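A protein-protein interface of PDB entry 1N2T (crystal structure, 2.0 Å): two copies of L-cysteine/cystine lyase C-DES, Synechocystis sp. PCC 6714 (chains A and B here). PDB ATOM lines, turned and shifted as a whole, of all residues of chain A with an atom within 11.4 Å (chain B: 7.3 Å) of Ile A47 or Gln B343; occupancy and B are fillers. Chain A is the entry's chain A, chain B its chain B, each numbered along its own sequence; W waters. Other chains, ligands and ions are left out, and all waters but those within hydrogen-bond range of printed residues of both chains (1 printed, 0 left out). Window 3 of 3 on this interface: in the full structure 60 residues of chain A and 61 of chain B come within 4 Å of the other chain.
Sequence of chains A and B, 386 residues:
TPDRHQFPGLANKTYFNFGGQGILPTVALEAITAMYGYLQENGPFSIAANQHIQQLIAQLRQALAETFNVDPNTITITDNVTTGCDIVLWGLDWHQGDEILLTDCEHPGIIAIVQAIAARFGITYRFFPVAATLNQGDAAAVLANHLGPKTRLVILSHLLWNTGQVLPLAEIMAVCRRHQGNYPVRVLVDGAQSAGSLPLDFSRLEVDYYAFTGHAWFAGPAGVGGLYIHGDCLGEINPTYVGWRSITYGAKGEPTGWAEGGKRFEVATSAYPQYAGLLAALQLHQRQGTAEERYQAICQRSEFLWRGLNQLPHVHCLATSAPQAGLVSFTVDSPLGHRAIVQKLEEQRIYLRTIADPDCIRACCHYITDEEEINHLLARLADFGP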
ATOM      1  N   MET A  35     -26.139 -12.072 -33.014  1.00  0.00           N
ATOM      2  CA  MET A  35     -24.920 -12.881 -33.146  1.00  0.00           C
ATOM      3  C   MET A  35     -23.692 -12.011 -33.376  1.00  0.00           C
ATOM      4  O   MET A  35     -22.601 -12.302 -32.869  1.00  0.00           O
ATOM      5  CB  MET A  35     -25.045 -13.904 -34.272  1.00  0.00           C
ATOM      6  CG  MET A  35     -25.265 -15.334 -33.787  1.00  0.00           C
ATOM      7  SD  MET A  35     -23.868 -16.008 -32.829  1.00  0.00           S
ATOM      8  CE  MET A  35     -22.750 -16.314 -34.003  1.00  0.00           C
ATOM      9  N   TYR A  38     -22.837 -10.785 -30.019  1.00  0.00           N
ATOM     10  CA  TYR A  38     -22.217 -11.796 -29.168  1.00  0.00           C
ATOM     11  C   TYR A  38     -20.744 -11.983 -29.541  1.00  0.00           C
ATOM     12  O   TYR A  38     -19.876 -12.085 -28.672  1.00  0.00           O
ATOM     13  CB  TYR A  38     -22.939 -13.146 -29.268  1.00  0.00           C
ATOM     14  CG  TYR A  38     -22.330 -14.201 -28.363  1.00  0.00           C
ATOM     15  CD1 TYR A  38     -21.161 -14.866 -28.721  1.00  0.00           C
ATOM     16  CD2 TYR A  38     -22.896 -14.488 -27.114  1.00  0.00           C
ATOM     17  CE1 TYR A  38     -20.562 -15.784 -27.867  1.00  0.00           C
ATOM     18  CE2 TYR A  38     -22.306 -15.410 -26.247  1.00  0.00           C
ATOM     19  CZ  TYR A  38     -21.137 -16.053 -26.628  1.00  0.00           C
ATOM     20  OH  TYR A  38     -20.538 -16.943 -25.763  1.00  0.00           O
ATOM     21  N   LEU A  39     -20.466 -12.038 -30.837  1.00  0.00           N
ATOM     22  CA  LEU A  39     -19.094 -12.203 -31.303  1.00  0.00           C
ATOM     23  C   LEU A  39     -18.224 -11.005 -30.936  1.00  0.00           C
ATOM     24  O   LEU A  39     -17.037 -11.156 -30.621  1.00  0.00           O
ATOM     25  CB  LEU A  39     -19.059 -12.410 -32.823  1.00  0.00           C
ATOM     26  CG  LEU A  39     -19.715 -13.697 -33.302  1.00  0.00           C
ATOM     27  CD1 LEU A  39     -19.744 -13.726 -34.828  1.00  0.00           C
ATOM     28  CD2 LEU A  39     -18.969 -14.900 -32.729  1.00  0.00           C
ATOM     29  N   GLU A  41     -18.675  -8.994 -28.320  1.00  0.00           N
ATOM     30  CA  GLU A  41     -18.490  -8.947 -26.877  1.00  0.00           C
ATOM     31  C   GLU A  41     -17.648 -10.050 -26.300  1.00  0.00           C
ATOM     32  O   GLU A  41     -16.948  -9.846 -25.308  1.00  0.00           O
ATOM     33  CB  GLU A  41     -19.856  -8.942 -26.180  1.00  0.00           C
ATOM     34  CG  GLU A  41     -20.622  -7.651 -26.395  1.00  0.00           C
ATOM     35  CD  GLU A  41     -19.925  -6.468 -25.740  1.00  0.00           C
ATOM     36  OE1 GLU A  41     -19.908  -5.371 -26.345  1.00  0.00           O
ATOM     37  OE2 GLU A  41     -19.396  -6.643 -24.617  1.00  0.00           O
ATOM     38  N   ASN A  42     -17.706 -11.219 -26.931  1.00  0.00           N
ATOM     39  CA  ASN A  42     -16.989 -12.381 -26.427  1.00  0.00           C
ATOM     40  C   ASN A  42     -15.815 -12.862 -27.261  1.00  0.00           C
ATOM     41  O   ASN A  42     -15.112 -13.754 -26.841  1.00  0.00           O
ATOM     42  CB  ASN A  42     -17.985 -13.530 -26.214  1.00  0.00           C
ATOM     43  CG  ASN A  42     -19.056 -13.180 -25.187  1.00  0.00           C
ATOM     44  OD1 ASN A  42     -18.832 -13.273 -23.981  1.00  0.00           O
ATOM     45  ND2 ASN A  42     -20.216 -12.754 -25.666  1.00  0.00           N
ATOM     46  N   GLY A  43     -15.583 -12.261 -28.420  1.00  0.00           N
ATOM     47  CA  GLY A  43     -14.459 -12.704 -29.227  1.00  0.00           C
ATOM     48  C   GLY A  43     -13.961 -11.607 -30.156  1.00  0.00           C
ATOM     49  O   GLY A  43     -13.459 -10.565 -29.684  1.00  0.00           O
ATOM     50  N   PRO A  44     -14.187 -11.744 -31.477  1.00  0.00           N
ATOM     51  CA  PRO A  44     -14.867 -12.813 -32.217  1.00  0.00           C
ATOM     52  C   PRO A  44     -14.237 -14.210 -32.302  1.00  0.00           C
ATOM     53  O   PRO A  44     -14.938 -15.185 -32.609  1.00  0.00           O
ATOM     54  CB  PRO A  44     -15.090 -12.177 -33.594  1.00  0.00           C
ATOM     55  CG  PRO A  44     -13.877 -11.292 -33.754  1.00  0.00           C
ATOM     56  CD  PRO A  44     -13.761 -10.660 -32.379  1.00  0.00           C
ATOM     57  N   PHE A  45     -12.937 -14.326 -32.035  1.00  0.00           N
ATOM     58  CA  PHE A  45     -12.272 -15.631 -32.080  1.00  0.00           C
ATOM     59  C   PHE A  45     -11.813 -15.921 -30.667  1.00  0.00           C
ATOM     60  O   PHE A  45     -10.952 -15.210 -30.136  1.00  0.00           O
ATOM     61  CB  PHE A  45     -11.039 -15.618 -33.014  1.00  0.00           C
ATOM     62  CG  PHE A  45     -10.458 -16.997 -33.278  1.00  0.00           C
ATOM     63  CD1 PHE A  45     -10.902 -17.757 -34.363  1.00  0.00           C
ATOM     64  CD2 PHE A  45      -9.508 -17.553 -32.413  1.00  0.00           C
ATOM     65  CE1 PHE A  45     -10.411 -19.067 -34.597  1.00  0.00           C
ATOM     66  CE2 PHE A  45      -9.012 -18.853 -32.632  1.00  0.00           C
ATOM     67  CZ  PHE A  45      -9.469 -19.616 -33.733  1.00  0.00           C
ATOM     68  N   SER A  46     -12.367 -16.965 -30.059  1.00  0.00           N
ATOM     69  CA  SER A  46     -12.016 -17.307 -28.691  1.00  0.00           C
ATOM     70  C   SER A  46     -12.698 -18.610 -28.305  1.00  0.00           C
ATOM     71  O   SER A  46     -13.523 -19.126 -29.051  1.00  0.00           O
ATOM     72  CB  SER A  46     -12.481 -16.201 -27.739  1.00  0.00           C
ATOM     73  OG  SER A  46     -13.898 -16.113 -27.722  1.00  0.00           O
ATOM     74  N   ILE A  47     -12.343 -19.134 -27.138  1.00  0.00           N
ATOM     75  CA  ILE A  47     -12.943 -20.360 -26.647  1.00  0.00           C
ATOM     76  C   ILE A  47     -14.456 -20.167 -26.532  1.00  0.00           C
ATOM     77  O   ILE A  47     -15.227 -20.973 -27.037  1.00  0.00           O
ATOM     78  CB  ILE A  47     -12.386 -20.752 -25.249  1.00  0.00           C
ATOM     79  CG1 ILE A  47     -10.871 -20.940 -25.309  1.00  0.00           C
ATOM     80  CG2 ILE A  47     -13.084 -22.019 -24.754  1.00  0.00           C
ATOM     81  CD1 ILE A  47     -10.210 -21.095 -23.928  1.00  0.00           C
ATOM     82  N   ALA A  48     -14.884 -19.091 -25.877  1.00  0.00           N
ATOM     83  CA  ALA A  48     -16.315 -18.835 -25.702  1.00  0.00           C
ATOM     84  C   ALA A  48     -17.041 -18.637 -27.039  1.00  0.00           C
ATOM     85  O   ALA A  48     -18.102 -19.216 -27.279  1.00  0.00           O
ATOM     86  CB  ALA A  48     -16.523 -17.618 -24.825  1.00  0.00           C
ATOM     87  N   ALA A  49     -16.474 -17.816 -27.915  1.00  0.00           N
ATOM     88  CA  ALA A  49     -17.108 -17.585 -29.210  1.00  0.00           C
ATOM     89  C   ALA A  49     -17.138 -18.858 -30.069  1.00  0.00           C
ATOM     90  O   ALA A  49     -18.174 -19.182 -30.658  1.00  0.00           O
ATOM     91  CB  ALA A  49     -16.400 -16.457 -29.960  1.00  0.00           C
ATOM     92  N   ASN A  50     -16.024 -19.573 -30.138  1.00  0.00           N
ATOM     93  CA  ASN A  50     -15.980 -20.801 -30.936  1.00  0.00           C
ATOM     94  C   ASN A  50     -16.976 -21.838 -30.420  1.00  0.00           C
ATOM     95  O   ASN A  50     -17.603 -22.552 -31.209  1.00  0.00           O
ATOM     96  CB  ASN A  50     -14.553 -21.369 -30.978  1.00  0.00           C
ATOM     97  CG  ASN A  50     -13.603 -20.479 -31.776  1.00  0.00           C
ATOM     98  OD1 ASN A  50     -14.038 -19.568 -32.475  1.00  0.00           O
ATOM     99  ND2 ASN A  50     -12.309 -20.740 -31.673  1.00  0.00           N
ATOM    100  N   GLN A  51     -17.148 -21.925 -29.105  1.00  0.00           N
ATOM    101  CA  GLN A  51     -18.125 -22.871 -28.561  1.00  0.00           C
ATOM    102  C   GLN A  51     -19.551 -22.443 -28.905  1.00  0.00           C
ATOM    103  O   GLN A  51     -20.413 -23.278 -29.205  1.00  0.00           O
ATOM    104  CB  GLN A  51     -18.028 -22.980 -27.041  1.00  0.00           C
ATOM    105  CG  GLN A  51     -19.284 -23.623 -26.461  1.00  0.00           C
ATOM    106  CD  GLN A  51     -19.216 -23.873 -24.975  1.00  0.00           C
ATOM    107  OE1 GLN A  51     -19.144 -22.937 -24.184  1.00  0.00           O
ATOM    108  NE2 GLN A  51     -19.248 -25.148 -24.584  1.00  0.00           N
ATOM    109  N   HIS A  52     -19.807 -21.140 -28.828  1.00  0.00           N
ATOM    110  CA  HIS A  52     -21.125 -20.587 -29.133  1.00  0.00           C
ATOM    111  C   HIS A  52     -21.500 -20.845 -30.608  1.00  0.00           C
ATOM    112  O   HIS A  52     -22.661 -21.112 -30.931  1.00  0.00           O
ATOM    113  CB  HIS A  52     -21.123 -19.091 -28.848  1.00  0.00           C
ATOM    114  CG  HIS A  52     -22.483 -18.476 -28.828  1.00  0.00           C
ATOM    115  ND1 HIS A  52     -23.393 -18.717 -27.822  1.00  0.00           N
ATOM    116  CD2 HIS A  52     -23.078 -17.597 -29.673  1.00  0.00           C
ATOM    117  CE1 HIS A  52     -24.488 -18.013 -28.042  1.00  0.00           C
ATOM    118  NE2 HIS A  52     -24.323 -17.323 -29.159  1.00  0.00           N
ATOM    119  N   ILE A  53     -20.510 -20.755 -31.490  1.00  0.00           N
ATOM    120  CA  ILE A  53     -20.699 -21.010 -32.914  1.00  0.00           C
ATOM    121  C   ILE A  53     -21.007 -22.492 -33.162  1.00  0.00           C
ATOM    122  O   ILE A  53     -21.920 -22.823 -33.916  1.00  0.00           O
ATOM    123  CB  ILE A  53     -19.441 -20.616 -33.716  1.00  0.00           C
ATOM    124  CG1 ILE A  53     -19.352 -19.090 -33.809  1.00  0.00           C
ATOM    125  CG2 ILE A  53     -19.467 -21.274 -35.123  1.00  0.00           C
ATOM    126  CD1 ILE A  53     -17.987 -18.582 -34.245  1.00  0.00           C
ATOM    127  N   GLN A  54     -20.244 -23.381 -32.533  1.00  0.00           N
ATOM    128  CA  GLN A  54     -20.485 -24.813 -32.691  1.00  0.00           C
ATOM    129  C   GLN A  54     -21.855 -25.210 -32.155  1.00  0.00           C
ATOM    130  O   GLN A  54     -22.522 -26.091 -32.710  1.00  0.00           O
ATOM    131  CB  GLN A  54     -19.406 -25.622 -31.982  1.00  0.00           C
ATOM    132  CG  GLN A  54     -18.145 -25.821 -32.798  1.00  0.00           C
ATOM    133  CD  GLN A  54     -17.213 -26.834 -32.156  1.00  0.00           C
ATOM    134  OE1 GLN A  54     -17.631 -27.945 -31.795  1.00  0.00           O
ATOM    135  NE2 GLN A  54     -15.941 -26.463 -32.013  1.00  0.00           N
ATOM    136  N   GLN A  55     -22.281 -24.579 -31.065  1.00  0.00           N
ATOM    137  CA  GLN A  55     -23.596 -24.881 -30.501  1.00  0.00           C
ATOM    138  C   GLN A  55     -24.698 -24.384 -31.453  1.00  0.00           C
ATOM    139  O   GLN A  55     -25.733 -25.049 -31.640  1.00  0.00           O
ATOM    140  CB  GLN A  55     -23.744 -24.235 -29.112  1.00  0.00           C
ATOM    141  CG  GLN A  55     -22.847 -24.867 -28.023  1.00  0.00           C
ATOM    142  CD  GLN A  55     -23.003 -24.188 -26.659  1.00  0.00           C
ATOM    143  OE1 GLN A  55     -23.115 -22.960 -26.566  1.00  0.00           O
ATOM    144  NE2 GLN A  55     -22.991 -24.986 -25.595  1.00  0.00           N
ATOM    145  N   LEU A  56     -24.480 -23.218 -32.055  1.00  0.00           N
ATOM    146  CA  LEU A  56     -25.460 -22.656 -32.997  1.00  0.00           C
ATOM    147  C   LEU A  56     -25.615 -23.571 -34.218  1.00  0.00           C
ATOM    148  O   LEU A  56     -26.730 -23.822 -34.691  1.00  0.00           O
ATOM    149  CB  LEU A  56     -25.031 -21.245 -33.449  1.00  0.00           C
ATOM    150  CG  LEU A  56     -25.775 -20.688 -34.684  1.00  0.00           C
ATOM    151  CD1 LEU A  56     -27.249 -20.558 -34.368  1.00  0.00           C
ATOM    152  CD2 LEU A  56     -25.207 -19.332 -35.092  1.00  0.00           C
ATOM    153  N   ASN B  17      -6.263 -11.973 -31.050  1.00  0.00           N
ATOM    154  CA  ASN B  17      -6.643 -13.075 -31.937  1.00  0.00           C
ATOM    155  C   ASN B  17      -7.047 -12.663 -33.359  1.00  0.00           C
ATOM    156  O   ASN B  17      -7.839 -13.343 -33.997  1.00  0.00           O
ATOM    157  CB  ASN B  17      -7.770 -13.920 -31.288  1.00  0.00           C
ATOM    158  CG  ASN B  17      -7.230 -15.000 -30.358  1.00  0.00           C
ATOM    159  OD1 ASN B  17      -6.066 -15.424 -30.471  1.00  0.00           O
ATOM    160  ND2 ASN B  17      -8.076 -15.467 -29.437  1.00  0.00           N
ATOM    161  N   GLY B 337       0.427 -26.327 -18.615  1.00  0.00           N
ATOM    162  CA  GLY B 337       0.145 -26.725 -19.984  1.00  0.00           C
ATOM    163  C   GLY B 337      -0.440 -25.518 -20.710  1.00  0.00           C
ATOM    164  O   GLY B 337      -1.213 -24.760 -20.126  1.00  0.00           O
ATOM    165  N   HIS B 338      -0.076 -25.341 -21.981  1.00  0.00           N
ATOM    166  CA  HIS B 338      -0.522 -24.201 -22.769  1.00  0.00           C
ATOM    167  C   HIS B 338      -2.027 -24.011 -22.936  1.00  0.00           C
ATOM    168  O   HIS B 338      -2.502 -22.880 -22.982  1.00  0.00           O
ATOM    169  CB  HIS B 338       0.169 -24.229 -24.135  1.00  0.00           C
ATOM    170  CG  HIS B 338       1.656 -24.089 -24.043  1.00  0.00           C
ATOM    171  ND1 HIS B 338       2.525 -24.818 -24.824  1.00  0.00           N
ATOM    172  CD2 HIS B 338       2.428 -23.298 -23.258  1.00  0.00           C
ATOM    173  CE1 HIS B 338       3.769 -24.483 -24.525  1.00  0.00           C
ATOM    174  NE2 HIS B 338       3.739 -23.564 -23.577  1.00  0.00           N
ATOM    175  N   ARG B 339      -2.794 -25.089 -23.021  1.00  0.00           N
ATOM    176  CA  ARG B 339      -4.230 -24.892 -23.170  1.00  0.00           C
ATOM    177  C   ARG B 339      -4.853 -24.354 -21.873  1.00  0.00           C
ATOM    178  O   ARG B 339      -5.752 -23.516 -21.910  1.00  0.00           O
ATOM    179  CB  ARG B 339      -4.916 -26.187 -23.632  1.00  0.00           C
ATOM    180  CG  ARG B 339      -4.462 -27.417 -22.909  1.00  0.00           C
ATOM    181  CD  ARG B 339      -5.177 -27.552 -21.588  1.00  0.00           C
ATOM    182  NE  ARG B 339      -4.363 -28.234 -20.584  1.00  0.00           N
ATOM    183  CZ  ARG B 339      -4.877 -28.931 -19.578  1.00  0.00           C
ATOM    184  NH1 ARG B 339      -6.197 -29.038 -19.455  1.00  0.00           N
ATOM    185  NH2 ARG B 339      -4.078 -29.512 -18.692  1.00  0.00           N
ATOM    186  N   ALA B 340      -4.365 -24.801 -20.721  1.00  0.00           N
ATOM    187  CA  ALA B 340      -4.932 -24.300 -19.479  1.00  0.00           C
ATOM    188  C   ALA B 340      -4.567 -22.828 -19.309  1.00  0.00           C
ATOM    189  O   ALA B 340      -5.363 -22.035 -18.792  1.00  0.00           O
ATOM    190  CB  ALA B 340      -4.432 -25.121 -18.300  1.00  0.00           C
ATOM    191  N   ILE B 341      -3.378 -22.456 -19.781  1.00  0.00           N
ATOM    192  CA  ILE B 341      -2.912 -21.078 -19.678  1.00  0.00           C
ATOM    193  C   ILE B 341      -3.764 -20.140 -20.534  1.00  0.00           C
ATOM    194  O   ILE B 341      -4.149 -19.069 -20.080  1.00  0.00           O
ATOM    195  CB  ILE B 341      -1.403 -20.962 -20.086  1.00  0.00           C
ATOM    196  CG1 ILE B 341      -0.525 -21.580 -18.994  1.00  0.00           C
ATOM    197  CG2 ILE B 341      -1.012 -19.496 -20.283  1.00  0.00           C
ATOM    198  CD1 ILE B 341       0.959 -21.619 -19.329  1.00  0.00           C
ATOM    199  N   VAL B 342      -4.068 -20.551 -21.766  1.00  0.00           N
ATOM    200  CA  VAL B 342      -4.897 -19.743 -22.667  1.00  0.00           C
ATOM    201  C   VAL B 342      -6.314 -19.573 -22.090  1.00  0.00           C
ATOM    202  O   VAL B 342      -6.919 -18.507 -22.206  1.00  0.00           O
ATOM    203  CB  VAL B 342      -4.969 -20.397 -24.081  1.00  0.00           C
ATOM    204  CG1 VAL B 342      -6.116 -19.820 -24.883  1.00  0.00           C
ATOM    205  CG2 VAL B 342      -3.652 -20.177 -24.821  1.00  0.00           C
ATOM    206  N   GLN B 343      -6.832 -20.622 -21.450  1.00  0.00           N
ATOM    207  CA  GLN B 343      -8.157 -20.567 -20.847  1.00  0.00           C
ATOM    208  C   GLN B 343      -8.182 -19.593 -19.667  1.00  0.00           C
ATOM    209  O   GLN B 343      -9.144 -18.832 -19.484  1.00  0.00           O
ATOM    210  CB  GLN B 343      -8.578 -21.960 -20.375  1.00  0.00           C
ATOM    211  CG  GLN B 343      -9.926 -21.984 -19.645  1.00  0.00           C
ATOM    212  CD  GLN B 343     -10.371 -23.399 -19.277  1.00  0.00           C
ATOM    213  OE1 GLN B 343     -11.289 -23.582 -18.482  1.00  0.00           O
ATOM    214  NE2 GLN B 343      -9.729 -24.391 -19.860  1.00  0.00           N
ATOM    215  N   LYS B 344      -7.122 -19.617 -18.865  1.00  0.00           N
ATOM    216  CA  LYS B 344      -7.024 -18.721 -17.717  1.00  0.00           C
ATOM    217  C   LYS B 344      -6.925 -17.275 -18.216  1.00  0.00           C
ATOM    218  O   LYS B 344      -7.512 -16.355 -17.625  1.00  0.00           O
ATOM    219  CB  LYS B 344      -5.788 -19.081 -16.880  1.00  0.00           C
ATOM    220  CG  LYS B 344      -5.697 -18.284 -15.582  1.00  0.00           C
ATOM    221  CD  LYS B 344      -6.934 -18.511 -14.707  1.00  0.00           C
ATOM    222  CE  LYS B 344      -7.092 -17.405 -13.661  1.00  0.00           C
ATOM    223  NZ  LYS B 344      -7.183 -16.069 -14.335  1.00  0.00           N
ATOM    224  N   LEU B 345      -6.179 -17.060 -19.300  1.00  0.00           N
ATOM    225  CA  LEU B 345      -6.062 -15.714 -19.855  1.00  0.00           C
ATOM    226  C   LEU B 345      -7.435 -15.234 -20.347  1.00  0.00           C
ATOM    227  O   LEU B 345      -7.817 -14.090 -20.107  1.00  0.00           O
ATOM    228  CB  LEU B 345      -5.034 -15.672 -20.997  1.00  0.00           C
ATOM    229  CG  LEU B 345      -3.560 -15.753 -20.561  1.00  0.00           C
ATOM    230  CD1 LEU B 345      -2.653 -15.880 -21.782  1.00  0.00           C
ATOM    231  CD2 LEU B 345      -3.201 -14.500 -19.773  1.00  0.00           C
ATOM    232  N   GLU B 346      -8.181 -16.107 -21.013  1.00  0.00           N
ATOM    233  CA  GLU B 346      -9.514 -15.730 -21.484  1.00  0.00           C
ATOM    234  C   GLU B 346     -10.428 -15.391 -20.283  1.00  0.00           C
ATOM    235  O   GLU B 346     -11.275 -14.492 -20.362  1.00  0.00           O
ATOM    236  CB  GLU B 346     -10.132 -16.860 -22.353  1.00  0.00           C
ATOM    237  CG  GLU B 346     -11.590 -16.592 -22.744  1.00  0.00           C
ATOM    238  CD  GLU B 346     -12.034 -17.246 -24.057  1.00  0.00           C
ATOM    239  OE1 GLU B 346     -13.263 -17.326 -24.274  1.00  0.00           O
ATOM    240  OE2 GLU B 346     -11.182 -17.658 -24.880  1.00  0.00           O
ATOM    241  N   GLU B 347     -10.255 -16.104 -19.171  1.00  0.00           N
ATOM    242  CA  GLU B 347     -11.043 -15.836 -17.965  1.00  0.00           C
ATOM    243  C   GLU B 347     -10.836 -14.380 -17.564  1.00  0.00           C
ATOM    244  O   GLU B 347     -11.699 -13.769 -16.935  1.00  0.00           O
ATOM    245  CB  GLU B 347     -10.593 -16.732 -16.799  1.00  0.00           C
ATOM    246  CG  GLU B 347     -10.998 -18.192 -16.909  1.00  0.00           C
ATOM    247  CD  GLU B 347     -12.475 -18.424 -16.630  1.00  0.00           C
ATOM    248  OE1 GLU B 347     -13.227 -17.429 -16.501  1.00  0.00           O
ATOM    249  OE2 GLU B 347     -12.885 -19.608 -16.548  1.00  0.00           O
ATOM    250  N   GLN B 348      -9.681 -13.833 -17.932  1.00  0.00           N
ATOM    251  CA  GLN B 348      -9.339 -12.443 -17.622  1.00  0.00           C
ATOM    252  C   GLN B 348      -9.595 -11.516 -18.806  1.00  0.00           C
ATOM    253  O   GLN B 348      -9.192 -10.355 -18.792  1.00  0.00           O
ATOM    254  CB  GLN B 348      -7.875 -12.367 -17.203  1.00  0.00           C
ATOM    255  CG  GLN B 348      -7.592 -13.118 -15.910  1.00  0.00           C
ATOM    256  CD  GLN B 348      -6.115 -13.242 -15.613  1.00  0.00           C
ATOM    257  OE1 GLN B 348      -5.405 -14.023 -16.250  1.00  0.00           O
ATOM    258  NE2 GLN B 348      -5.640 -12.467 -14.648  1.00  0.00           N
ATOM    259  N   ARG B 349     -10.291 -12.040 -19.812  1.00  0.00           N
ATOM    260  CA  ARG B 349     -10.624 -11.299 -21.022  1.00  0.00           C
ATOM    261  C   ARG B 349      -9.404 -10.882 -21.831  1.00  0.00           C
ATOM    262  O   ARG B 349      -9.357  -9.806 -22.414  1.00  0.00           O
ATOM    263  CB  ARG B 349     -11.523 -10.088 -20.705  1.00  0.00           C
ATOM    264  CG  ARG B 349     -12.931 -10.495 -20.252  1.00  0.00           C
ATOM    265  CD  ARG B 349     -13.853  -9.297 -19.988  1.00  0.00           C
ATOM    266  NE  ARG B 349     -14.297  -8.630 -21.213  1.00  0.00           N
ATOM    267  CZ  ARG B 349     -15.216  -9.116 -22.052  1.00  0.00           C
ATOM    268  NH1 ARG B 349     -15.797 -10.279 -21.802  1.00  0.00           N
ATOM    269  NH2 ARG B 349     -15.552  -8.442 -23.153  1.00  0.00           N
ATOM    270  N   ILE B 350      -8.415 -11.770 -21.853  1.00  0.00           N
ATOM    271  CA  ILE B 350      -7.192 -11.598 -22.630  1.00  0.00           C
ATOM    272  C   ILE B 350      -7.267 -12.774 -23.633  1.00  0.00           C
ATOM    273  O   ILE B 350      -7.270 -13.950 -23.240  1.00  0.00           O
ATOM    274  CB  ILE B 350      -5.970 -11.714 -21.736  1.00  0.00           C
ATOM    275  CG1 ILE B 350      -6.038 -10.614 -20.666  1.00  0.00           C
ATOM    276  CG2 ILE B 350      -4.704 -11.557 -22.555  1.00  0.00           C
ATOM    277  CD1 ILE B 350      -4.918 -10.669 -19.654  1.00  0.00           C
ATOM    278  N   TYR B 351      -7.315 -12.448 -24.922  1.00  0.00           N
ATOM    279  CA  TYR B 351      -7.498 -13.463 -25.962  1.00  0.00           C
ATOM    280  C   TYR B 351      -6.334 -13.834 -26.878  1.00  0.00           C
ATOM    281  O   TYR B 351      -5.945 -13.041 -27.722  1.00  0.00           O
ATOM    282  CB  TYR B 351      -8.680 -13.036 -26.833  1.00  0.00           C
ATOM    283  CG  TYR B 351      -9.966 -12.833 -26.057  1.00  0.00           C
ATOM    284  CD1 TYR B 351     -10.226 -11.640 -25.377  1.00  0.00           C
ATOM    285  CD2 TYR B 351     -10.896 -13.860 -25.950  1.00  0.00           C
ATOM    286  CE1 TYR B 351     -11.384 -11.487 -24.601  1.00  0.00           C
ATOM    287  CE2 TYR B 351     -12.048 -13.719 -25.186  1.00  0.00           C
ATOM    288  CZ  TYR B 351     -12.284 -12.540 -24.512  1.00  0.00           C
ATOM    289  OH  TYR B 351     -13.398 -12.425 -23.718  1.00  0.00           O
ATOM    290  N   LEU B 352      -5.801 -15.041 -26.695  1.00  0.00           N
ATOM    291  CA  LEU B 352      -4.721 -15.593 -27.518  1.00  0.00           C
ATOM    292  C   LEU B 352      -5.168 -17.008 -27.907  1.00  0.00           C
ATOM    293  O   LEU B 352      -6.298 -17.412 -27.605  1.00  0.00           O
ATOM    294  CB  LEU B 352      -3.396 -15.681 -26.747  1.00  0.00           C
ATOM    295  CG  LEU B 352      -2.639 -14.364 -26.488  1.00  0.00           C
ATOM    296  CD1 LEU B 352      -3.412 -13.529 -25.478  1.00  0.00           C
ATOM    297  CD2 LEU B 352      -1.235 -14.651 -25.966  1.00  0.00           C
ATOM    298  N   THR B 354      -3.961 -21.396 -28.679  1.00  0.00           N
ATOM    299  CA  THR B 354      -2.986 -22.483 -28.606  1.00  0.00           C
ATOM    300  C   THR B 354      -2.713 -22.983 -30.027  1.00  0.00           C
ATOM    301  O   THR B 354      -3.604 -22.939 -30.889  1.00  0.00           O
ATOM    302  CB  THR B 354      -3.529 -23.662 -27.772  1.00  0.00           C
ATOM    303  OG1 THR B 354      -3.804 -23.210 -26.440  1.00  0.00           O
ATOM    304  CG2 THR B 354      -2.504 -24.767 -27.681  1.00  0.00           C
HETATM  305  O   HOH W   1     -18.540 -11.169 -22.278  1.00  0.00           O
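The backbone carbonyl oxygen of Tyr A38 lies within hydrogen-bond range of the side-chain amide nitrogen of Asn A42, at 3.1 Å.
The backbone carbonyl oxygen (O) of Asn A42 lies within hydrogen-bond range of the side-chain hydroxyl (OG) of Ser A46, 2.8 Å away.
The backbone NH of Ala A49 is in hydrogen-bond range of the side-chain hydroxyl of Ser A46.
ND2 of Asn A50 lies close to O of Ser A46, at 3.3 Å.
ND2 of Asn B17 is in hydrogen-bond range of O of Leu B352 (3.2 Å).
Of the printed residues of chain B, Asn A42 touches Tyr B351.
Printed residues of chain B within 4 Å of Phe A45: Asn B17.
Printed residues of chain B within 4 Å of Ser A46: Glu B346 (3.5 Å) and Tyr B351 (3.3 Å).
Of chain A, only Ile A47 (3.7 Å) comes within 4 Å of Gln B343.
No residue of chain A comes within 4 Å of Lys B344.
No residue of chain A comes within 4 Å of Leu B345.
Of chain A, only Ser A46 (3.5 Å), Ile A47 (2.9 Å) and Ala A48 (2.9 Å) come within 4 Å of Glu B346.
No residue of chain A comes within 4 Å of Glu B347.
The nearest residue of chain A that does not touch Gln B343 is Ala A48 (8.5 Å).
The guanidinium group of Arg B349 sits at hydrogen-bond distance from the backbone carbonyl oxygen of Glu A41, 2.9 Å away.
The side-chain amide nitrogen of Asn B17 is in hydrogen-bond range of the backbone carbonyl oxygen of Phe A45.
The backbone NH of Ile A47 is in hydrogen-bond range of the side-chain carboxylate of Glu B346 (2.9 Å).
The backbone NH of Ala A48 lies within hydrogen-bond range of the side-chain carboxylate of Glu B346, 2.9 Å away.
No position is printed for both chains.
Among the printed residues, merely in contact across the chains: Asn A42 with Tyr B351, Ser A46 with Glu B346, Ser A46 with Tyr B351 and Ile A47 with Gln B343.
Hydrophobic or aromatic side chains of chain A within 4 Å of the printed part of chain B: Phe A45, Ile A47 and Ala A48.
Hydrophobic or aromatic side chains of chain B that line the printed part of chain A: Tyr B351.
Among the printed residues, no Asp or Glu carboxylate lies within 4 Å of a Lys or Arg side-chain nitrogen of the other chain.
Water W1 bridges the side-chain amide oxygen of Asn A42 and the guanidinium group of Arg B349.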
